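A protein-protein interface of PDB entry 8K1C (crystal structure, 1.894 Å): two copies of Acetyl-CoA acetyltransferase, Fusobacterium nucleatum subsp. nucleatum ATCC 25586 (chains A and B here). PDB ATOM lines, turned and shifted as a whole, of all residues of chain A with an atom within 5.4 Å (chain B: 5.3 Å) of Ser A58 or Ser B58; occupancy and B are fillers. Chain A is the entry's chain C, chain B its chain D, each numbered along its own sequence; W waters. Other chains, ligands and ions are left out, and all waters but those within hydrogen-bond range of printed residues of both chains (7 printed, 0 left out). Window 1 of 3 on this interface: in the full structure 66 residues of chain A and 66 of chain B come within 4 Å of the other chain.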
ATOM      1  N   ASN A  55       4.787  -5.901 -29.781  1.00  0.00           N
ATOM      2  CA  ASN A  55       6.178  -6.332 -29.874  1.00  0.00           C
ATOM      3  C   ASN A  55       6.998  -5.490 -28.909  1.00  0.00           C
ATOM      4  O   ASN A  55       6.868  -4.262 -28.885  1.00  0.00           O
ATOM      5  CB  ASN A  55       6.683  -6.205 -31.320  1.00  0.00           C
ATOM      6  CG  ASN A  55       8.172  -6.522 -31.471  1.00  0.00           C
ATOM      7  OD1 ASN A  55       8.957  -5.648 -31.848  1.00  0.00           O
ATOM      8  ND2 ASN A  55       8.557  -7.782 -31.221  1.00  0.00           N
ATOM      9  N   VAL A  56       7.808  -6.137 -28.078  1.00  0.00           N
ATOM     10  CA  VAL A  56       8.588  -5.452 -27.046  1.00  0.00           C
ATOM     11  C   VAL A  56      10.048  -5.297 -27.458  1.00  0.00           C
ATOM     12  O   VAL A  56      10.634  -4.220 -27.333  1.00  0.00           O
ATOM     13  CB  VAL A  56       8.476  -6.207 -25.702  1.00  0.00           C
ATOM     14  CG1 VAL A  56       9.321  -5.503 -24.620  1.00  0.00           C
ATOM     15  CG2 VAL A  56       7.025  -6.328 -25.286  1.00  0.00           C
ATOM     16  N   LEU A  57      10.658  -6.374 -27.944  1.00  0.00           N
ATOM     17  CA  LEU A  57      12.100  -6.410 -28.185  1.00  0.00           C
ATOM     18  C   LEU A  57      12.337  -6.122 -29.670  1.00  0.00           C
ATOM     19  O   LEU A  57      12.491  -7.021 -30.498  1.00  0.00           O
ATOM     20  CB  LEU A  57      12.669  -7.760 -27.741  1.00  0.00           C
ATOM     21  CG  LEU A  57      12.450  -8.115 -26.263  1.00  0.00           C
ATOM     22  CD1 LEU A  57      12.834  -9.546 -25.987  1.00  0.00           C
ATOM     23  CD2 LEU A  57      13.249  -7.182 -25.332  1.00  0.00           C
ATOM     24  N   SER A  58      12.356  -4.834 -30.002  1.00  0.00           N
ATOM     25  CA  SER A  58      12.397  -4.394 -31.389  1.00  0.00           C
ATOM     26  C   SER A  58      13.807  -4.141 -31.892  1.00  0.00           C
ATOM     27  O   SER A  58      13.970  -3.795 -33.064  1.00  0.00           O
ATOM     28  CB  SER A  58      11.590  -3.108 -31.561  1.00  0.00           C
ATOM     29  OG  SER A  58      11.901  -2.195 -30.519  1.00  0.00           O
ATOM     30  N   ALA A  59      14.817  -4.280 -31.040  1.00  0.00           N
ATOM     31  CA  ALA A  59      16.186  -3.942 -31.420  1.00  0.00           C
ATOM     32  C   ALA A  59      16.760  -4.951 -32.408  1.00  0.00           C
ATOM     33  O   ALA A  59      16.596  -6.165 -32.258  1.00  0.00           O
ATOM     34  CB  ALA A  59      17.078  -3.870 -30.180  1.00  0.00           C
ATOM     35  N   GLY A  60      17.463  -4.439 -33.415  1.00  0.00           N
ATOM     36  CA  GLY A  60      18.131  -5.309 -34.361  1.00  0.00           C
ATOM     37  C   GLY A  60      17.230  -5.912 -35.404  1.00  0.00           C
ATOM     38  O   GLY A  60      17.627  -6.885 -36.053  1.00  0.00           O
ATOM     39  N   GLN A  61      16.010  -5.396 -35.579  1.00  0.00           N
ATOM     40  CA  GLN A  61      15.056  -6.010 -36.538  1.00  0.00           C
ATOM     41  C   GLN A  61      14.967  -5.209 -37.849  1.00  0.00           C
ATOM     42  O   GLN A  61      14.246  -5.590 -38.711  1.00  0.00           O
ATOM     43  CB  GLN A  61      13.655  -6.050 -35.911  1.00  0.00           C
ATOM     44  CG  GLN A  61      13.544  -6.921 -34.678  1.00  0.00           C
ATOM     45  CD  GLN A  61      14.092  -8.312 -34.896  1.00  0.00           C
ATOM     46  OE1 GLN A  61      13.904  -8.900 -35.935  1.00  0.00           O
ATOM     47  NE2 GLN A  61      14.773  -8.851 -33.908  1.00  0.00           N
ATOM     48  N   ALA A  62      15.557  -4.015 -37.824  1.00  0.00           N
ATOM     49  CA  ALA A  62      15.422  -2.940 -38.840  1.00  0.00           C
ATOM     50  C   ALA A  62      14.043  -2.263 -38.646  1.00  0.00           C
ATOM     51  O   ALA A  62      13.337  -2.581 -37.711  1.00  0.00           O
ATOM     52  CB  ALA A  62      15.750  -3.304 -40.266  1.00  0.00           C
ATOM     53  N   VAL A  65       8.718  -3.746 -36.711  1.00  0.00           N
ATOM     54  CA  VAL A  65       8.311  -5.168 -36.713  1.00  0.00           C
ATOM     55  C   VAL A  65       6.853  -5.277 -37.211  1.00  0.00           C
ATOM     56  O   VAL A  65       6.572  -6.162 -37.968  1.00  0.00           O
ATOM     57  CB  VAL A  65       8.541  -5.740 -35.307  1.00  0.00           C
ATOM     58  CG1 VAL A  65       7.958  -7.106 -35.112  1.00  0.00           C
ATOM     59  CG2 VAL A  65      10.000  -5.707 -34.900  1.00  0.00           C
ATOM     60  N   ASN A  85       4.021  -1.183 -27.720  1.00  0.00           N
ATOM     61  CA  ASN A  85       4.792  -1.791 -26.638  1.00  0.00           C
ATOM     62  C   ASN A  85       4.210  -1.311 -25.314  1.00  0.00           C
ATOM     63  O   ASN A  85       4.484  -0.191 -24.866  1.00  0.00           O
ATOM     64  CB  ASN A  85       6.285  -1.474 -26.748  1.00  0.00           C
ATOM     65  CG  ASN A  85       7.097  -2.042 -25.579  1.00  0.00           C
ATOM     66  OD1 ASN A  85       6.554  -2.727 -24.700  1.00  0.00           O
ATOM     67  ND2 ASN A  85       8.405  -1.772 -25.576  1.00  0.00           N
ATOM     68  N   HIS A 143      19.358  -7.507 -23.996  1.00  0.00           N
ATOM     69  CA  HIS A 143      18.180  -6.776 -24.467  1.00  0.00           C
ATOM     70  C   HIS A 143      16.894  -7.393 -23.925  1.00  0.00           C
ATOM     71  O   HIS A 143      15.964  -6.666 -23.556  1.00  0.00           O
ATOM     72  CB  HIS A 143      18.179  -6.743 -26.007  1.00  0.00           C
ATOM     73  CG  HIS A 143      16.977  -6.081 -26.637  1.00  0.00           C
ATOM     74  ND1 HIS A 143      16.397  -4.930 -26.140  1.00  0.00           N
ATOM     75  CD2 HIS A 143      16.277  -6.395 -27.759  1.00  0.00           C
ATOM     76  CE1 HIS A 143      15.386  -4.575 -26.918  1.00  0.00           C
ATOM     77  NE2 HIS A 143      15.292  -5.447 -27.905  1.00  0.00           N
ATOM     78  N   ASP A 147      15.045  -4.995 -21.245  1.00  0.00           N
ATOM     79  CA  ASP A 147      13.931  -4.289 -21.863  1.00  0.00           C
ATOM     80  C   ASP A 147      12.601  -5.026 -21.765  1.00  0.00           C
ATOM     81  O   ASP A 147      11.549  -4.374 -21.813  1.00  0.00           O
ATOM     82  CB  ASP A 147      14.292  -3.968 -23.321  1.00  0.00           C
ATOM     83  CG  ASP A 147      15.468  -3.004 -23.406  1.00  0.00           C
ATOM     84  OD1 ASP A 147      15.450  -1.985 -22.672  1.00  0.00           O
ATOM     85  OD2 ASP A 147      16.423  -3.270 -24.163  1.00  0.00           O
ATOM     86  N   ASN B  55       7.801   6.309 -29.748  1.00  0.00           N
ATOM     87  CA  ASN B  55       9.219   6.063 -29.473  1.00  0.00           C
ATOM     88  C   ASN B  55       9.703   4.920 -30.351  1.00  0.00           C
ATOM     89  O   ASN B  55       9.055   3.867 -30.408  1.00  0.00           O
ATOM     90  CB  ASN B  55       9.445   5.731 -27.993  1.00  0.00           C
ATOM     91  CG  ASN B  55      10.888   5.340 -27.688  1.00  0.00           C
ATOM     92  OD1 ASN B  55      11.154   4.226 -27.220  1.00  0.00           O
ATOM     93  ND2 ASN B  55      11.818   6.260 -27.922  1.00  0.00           N
ATOM     94  N   VAL B  56      10.823   5.128 -31.039  1.00  0.00           N
ATOM     95  CA  VAL B  56      11.335   4.150 -31.997  1.00  0.00           C
ATOM     96  C   VAL B  56      12.469   3.325 -31.409  1.00  0.00           C
ATOM     97  O   VAL B  56      12.479   2.101 -31.532  1.00  0.00           O
ATOM     98  CB  VAL B  56      11.783   4.844 -33.306  1.00  0.00           C
ATOM     99  CG1 VAL B  56      12.326   3.792 -34.284  1.00  0.00           C
ATOM    100  CG2 VAL B  56      10.625   5.659 -33.928  1.00  0.00           C
ATOM    101  N   LEU B  57      13.434   3.984 -30.766  1.00  0.00           N
ATOM    102  CA  LEU B  57      14.693   3.357 -30.356  1.00  0.00           C
ATOM    103  C   LEU B  57      14.614   3.011 -28.868  1.00  0.00           C
ATOM    104  O   LEU B  57      15.053   3.758 -27.990  1.00  0.00           O
ATOM    105  CB  LEU B  57      15.855   4.289 -30.682  1.00  0.00           C
ATOM    106  CG  LEU B  57      15.924   4.623 -32.178  1.00  0.00           C
ATOM    107  CD1 LEU B  57      16.900   5.754 -32.461  1.00  0.00           C
ATOM    108  CD2 LEU B  57      16.279   3.386 -32.988  1.00  0.00           C
ATOM    109  N   SER B  58      14.033   1.845 -28.590  1.00  0.00           N
ATOM    110  CA  SER B  58      13.666   1.460 -27.233  1.00  0.00           C
ATOM    111  C   SER B  58      14.684   0.542 -26.581  1.00  0.00           C
ATOM    112  O   SER B  58      14.510   0.183 -25.412  1.00  0.00           O
ATOM    113  CB  SER B  58      12.290   0.782 -27.226  1.00  0.00           C
ATOM    114  OG  SER B  58      12.301  -0.377 -28.042  1.00  0.00           O
ATOM    115  N   ALA B  59      15.744   0.172 -27.291  1.00  0.00           N
ATOM    116  CA  ALA B  59      16.751  -0.708 -26.722  1.00  0.00           C
ATOM    117  C   ALA B  59      17.534  -0.004 -25.622  1.00  0.00           C
ATOM    118  O   ALA B  59      17.910   1.163 -25.756  1.00  0.00           O
ATOM    119  CB  ALA B  59      17.702  -1.194 -27.807  1.00  0.00           C
ATOM    120  N   GLY B  60      17.782  -0.727 -24.531  1.00  0.00           N
ATOM    121  CA  GLY B  60      18.629  -0.237 -23.460  1.00  0.00           C
ATOM    122  C   GLY B  60      17.972   0.705 -22.482  1.00  0.00           C
ATOM    123  O   GLY B  60      18.680   1.358 -21.712  1.00  0.00           O
ATOM    124  N   GLN B  61      16.616   0.667 -22.529  1.00  0.00           N
ATOM    125  CA  GLN B  61      16.056   1.715 -21.643  1.00  0.00           C
ATOM    126  C   GLN B  61      15.419   1.135 -20.386  1.00  0.00           C
ATOM    127  O   GLN B  61      14.875   1.880 -19.632  1.00  0.00           O
ATOM    128  CB  GLN B  61      14.940   2.447 -22.382  1.00  0.00           C
ATOM    129  CG  GLN B  61      15.439   3.237 -23.576  1.00  0.00           C
ATOM    130  CD  GLN B  61      16.442   4.283 -23.151  1.00  0.00           C
ATOM    131  OE1 GLN B  61      16.284   4.925 -22.132  1.00  0.00           O
ATOM    132  NE2 GLN B  61      17.476   4.466 -23.947  1.00  0.00           N
ATOM    133  N   ALA B  62      15.301  -0.185 -20.368  1.00  0.00           N
ATOM    134  CA  ALA B  62      14.478  -0.965 -19.417  1.00  0.00           C
ATOM    135  C   ALA B  62      12.991  -0.866 -19.840  1.00  0.00           C
ATOM    136  O   ALA B  62      12.670  -0.237 -20.859  1.00  0.00           O
ATOM    137  CB  ALA B  62      14.763  -0.773 -17.949  1.00  0.00           C
ATOM    138  N   VAL B  65       9.377   2.827 -22.324  1.00  0.00           N
ATOM    139  CA  VAL B  65       9.734   4.257 -22.350  1.00  0.00           C
ATOM    140  C   VAL B  65       8.456   5.062 -22.076  1.00  0.00           C
ATOM    141  O   VAL B  65       8.502   5.978 -21.304  1.00  0.00           O
ATOM    142  CB  VAL B  65      10.337   4.608 -23.718  1.00  0.00           C
ATOM    143  CG1 VAL B  65      10.261   6.078 -24.008  1.00  0.00           C
ATOM    144  CG2 VAL B  65      11.750   4.079 -23.864  1.00  0.00           C
ATOM    145  N   ASN B  85       5.208   2.495 -32.047  1.00  0.00           N
ATOM    146  CA  ASN B  85       6.302   2.577 -33.017  1.00  0.00           C
ATOM    147  C   ASN B  85       5.784   2.401 -34.446  1.00  0.00           C
ATOM    148  O   ASN B  85       5.528   1.291 -34.826  1.00  0.00           O
ATOM    149  CB  ASN B  85       7.430   1.599 -32.707  1.00  0.00           C
ATOM    150  CG  ASN B  85       8.555   1.678 -33.713  1.00  0.00           C
ATOM    151  OD1 ASN B  85       8.520   2.515 -34.579  1.00  0.00           O
ATOM    152  ND2 ASN B  85       9.525   0.793 -33.613  1.00  0.00           N
ATOM    153  N   HIS B 143      22.052   0.822 -33.510  1.00  0.00           N
ATOM    154  CA  HIS B 143      20.617   0.774 -33.214  1.00  0.00           C
ATOM    155  C   HIS B 143      19.856   1.889 -33.933  1.00  0.00           C
ATOM    156  O   HIS B 143      18.798   1.649 -34.532  1.00  0.00           O
ATOM    157  CB  HIS B 143      20.440   0.855 -31.689  1.00  0.00           C
ATOM    158  CG  HIS B 143      19.020   0.794 -31.211  1.00  0.00           C
ATOM    159  ND1 HIS B 143      18.063  -0.014 -31.791  1.00  0.00           N
ATOM    160  CD2 HIS B 143      18.409   1.417 -30.173  1.00  0.00           C
ATOM    161  CE1 HIS B 143      16.919   0.128 -31.143  1.00  0.00           C
ATOM    162  NE2 HIS B 143      17.101   0.993 -30.159  1.00  0.00           N
ATOM    163  N   ASP B 147      17.469   0.430 -36.869  1.00  0.00           N
ATOM    164  CA  ASP B 147      16.082   0.327 -36.445  1.00  0.00           C
ATOM    165  C   ASP B 147      15.263   1.602 -36.673  1.00  0.00           C
ATOM    166  O   ASP B 147      14.029   1.524 -36.762  1.00  0.00           O
ATOM    167  CB  ASP B 147      16.049  -0.110 -34.983  1.00  0.00           C
ATOM    168  CG  ASP B 147      16.616  -1.521 -34.792  1.00  0.00           C
ATOM    169  OD1 ASP B 147      16.326  -2.409 -35.633  1.00  0.00           O
ATOM    170  OD2 ASP B 147      17.356  -1.745 -33.812  1.00  0.00           O
HETATM  171  O   HOH W   1       9.859   0.931 -24.187  1.00  0.00           O
HETATM  172  O   HOH W   2       9.875  -2.280 -34.818  1.00  0.00           O
HETATM  173  O   HOH W   3       6.079   1.961 -23.060  1.00  0.00           O
HETATM  174  O   HOH W   4       6.199  -1.479 -36.721  1.00  0.00           O
HETATM  175  O   HOH W   5      10.485   0.160 -30.652  1.00  0.00           O
HETATM  176  O   HOH W   6       6.289   0.201 -29.836  1.00  0.00           O
HETATM  177  O   HOH W   7       9.734  -1.569 -28.142  1.00  0.00           O
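The side-chain hydroxyl (OG) of Ser B58 lies within hydrogen-bond range of the side-chain hydroxyl (OG) of Ser A58 (3.1 Å). The backbone NH (N) of Gly A60 is in hydrogen-bond range of the side-chain carboxylate (OD2) of Asp B147 (2.7 Å). The backbone NH (N) of Gln A61 sits at hydrogen-bond distance from the side-chain carboxylate (OD1) of Asp B147, at 3.0 Å. The backbone NH of Ala A62 sits at hydrogen-bond distance from the side-chain carboxylate of Asp B147, at 2.8 Å. The side-chain carboxylate (OD2) of Asp A147 lies within hydrogen-bond range of the backbone NH (N) of Gly B60 (2.9 Å). N of Gln B61 lies within hydrogen-bond range of OD1 of Asp A147, at 2.9 Å. The backbone NH (N) of Ala B62 is in hydrogen-bond range of the side-chain carboxylate (OD1) of Asp A147.
A ring nitrogen (NE2) of His A143 sits close to the backbone NH (N) of Ala A59. ND1 of His A143 is in hydrogen-bond range of OD2 of Asp A147. The backbone NH (N) of Ala B59 lies close to a ring nitrogen (NE2) of His B143. A ring nitrogen (ND1) of His B143 sits at hydrogen-bond distance from the side-chain carboxylate (OD2) of Asp B147 (2.8 Å).
OD1 of Asp B147 touches O of Ser A58, 3.8 Å away. CB of Ala B59 touches CB of Ala A59 (3.6 Å). Ala A59 touches Asp B147. Ser B58 touches Asp A147 (O to OD1, 3.6 Å). Ala B59 touches Asp A147.
Ser A58 touches just these residues of chain B: Ser B58 (3.1 Å) and Asp B147 (3.8 Å). Ser B58 touches two residues of chain A. Of the printed residues of chain B, Asp A147 touches Ser B58 (3.6 Å), Ala B59 (3.6 Å), Gly B60 (2.9 Å), Gln B61 (2.9 Å) and Ala B62 (2.9 Å). Of the printed residues of chain A, Asp B147 touches Ser A58, Ala A59, Gly A60, Gln A61 and Ala A62. Asn B85 touches none of the printed residues of chain A. Asn B55 touches none of the printed residues of chain A. The nearest residue of chain A that does not touch Ser B58 is Val A56 (4.2 Å).
Of the 12 printed residues of chain B, 6 touch a printed residue of chain A. Hydrophobic or aromatic side chains of chain B that line the printed part of chain A: Ala B59. Among the printed residues, 12 pairs touch across the chains.
Ser A58 touches its own counterpart, Ser B58. Ser A58 touches Asp B147, and with the chains exchanged Asp A147 touches Ser B58. Ala A59 touches its own counterpart, Ala B59. Gly A60 touches Asp B147, and with the chains exchanged Asp A147 touches Gly B60. 12 positions are printed for both chains. Of the 12 pairs that touch across the chains among the printed residues, 12 have their exchanged pair printed and touching as well.
Water W1 lies within hydrogen-bond range of N of Val B65 (2.7 Å) and ND2 of Asn A85 (3.4 Å). Water W5 lies within hydrogen-bond range of the side-chain hydroxyl (OG) of Ser A58 (2.8 Å), the backbone carbonyl oxygen (O) of Val B56 (2.9 Å), the side-chain amide nitrogen (ND2) of Asn B85 (3.2 Å) and the side-chain hydroxyl (OG) of Ser B58 (3.2 Å). Water W7 lies within hydrogen-bond range of the side-chain hydroxyl (OG) of Ser B58 (2.8 Å), the side-chain amide nitrogen (ND2) of Asn A85 (2.9 Å), the backbone carbonyl oxygen (O) of Val A56 (2.9 Å) and the side-chain hydroxyl (OG) of Ser A58 (3.3 Å). Water W3 lies within hydrogen-bond range of the backbone carbonyl oxygen of Asn A85 (3.2 Å) and the backbone NH of Val B65 (3.5 Å). Water W6 lies within hydrogen-bond range of the backbone NH (N) of Asn B85 and the backbone NH (N) of Asn A85. Water W4 bridges N of Val A65 (3.4 Å) and O of Asn B85 (3.4 Å).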
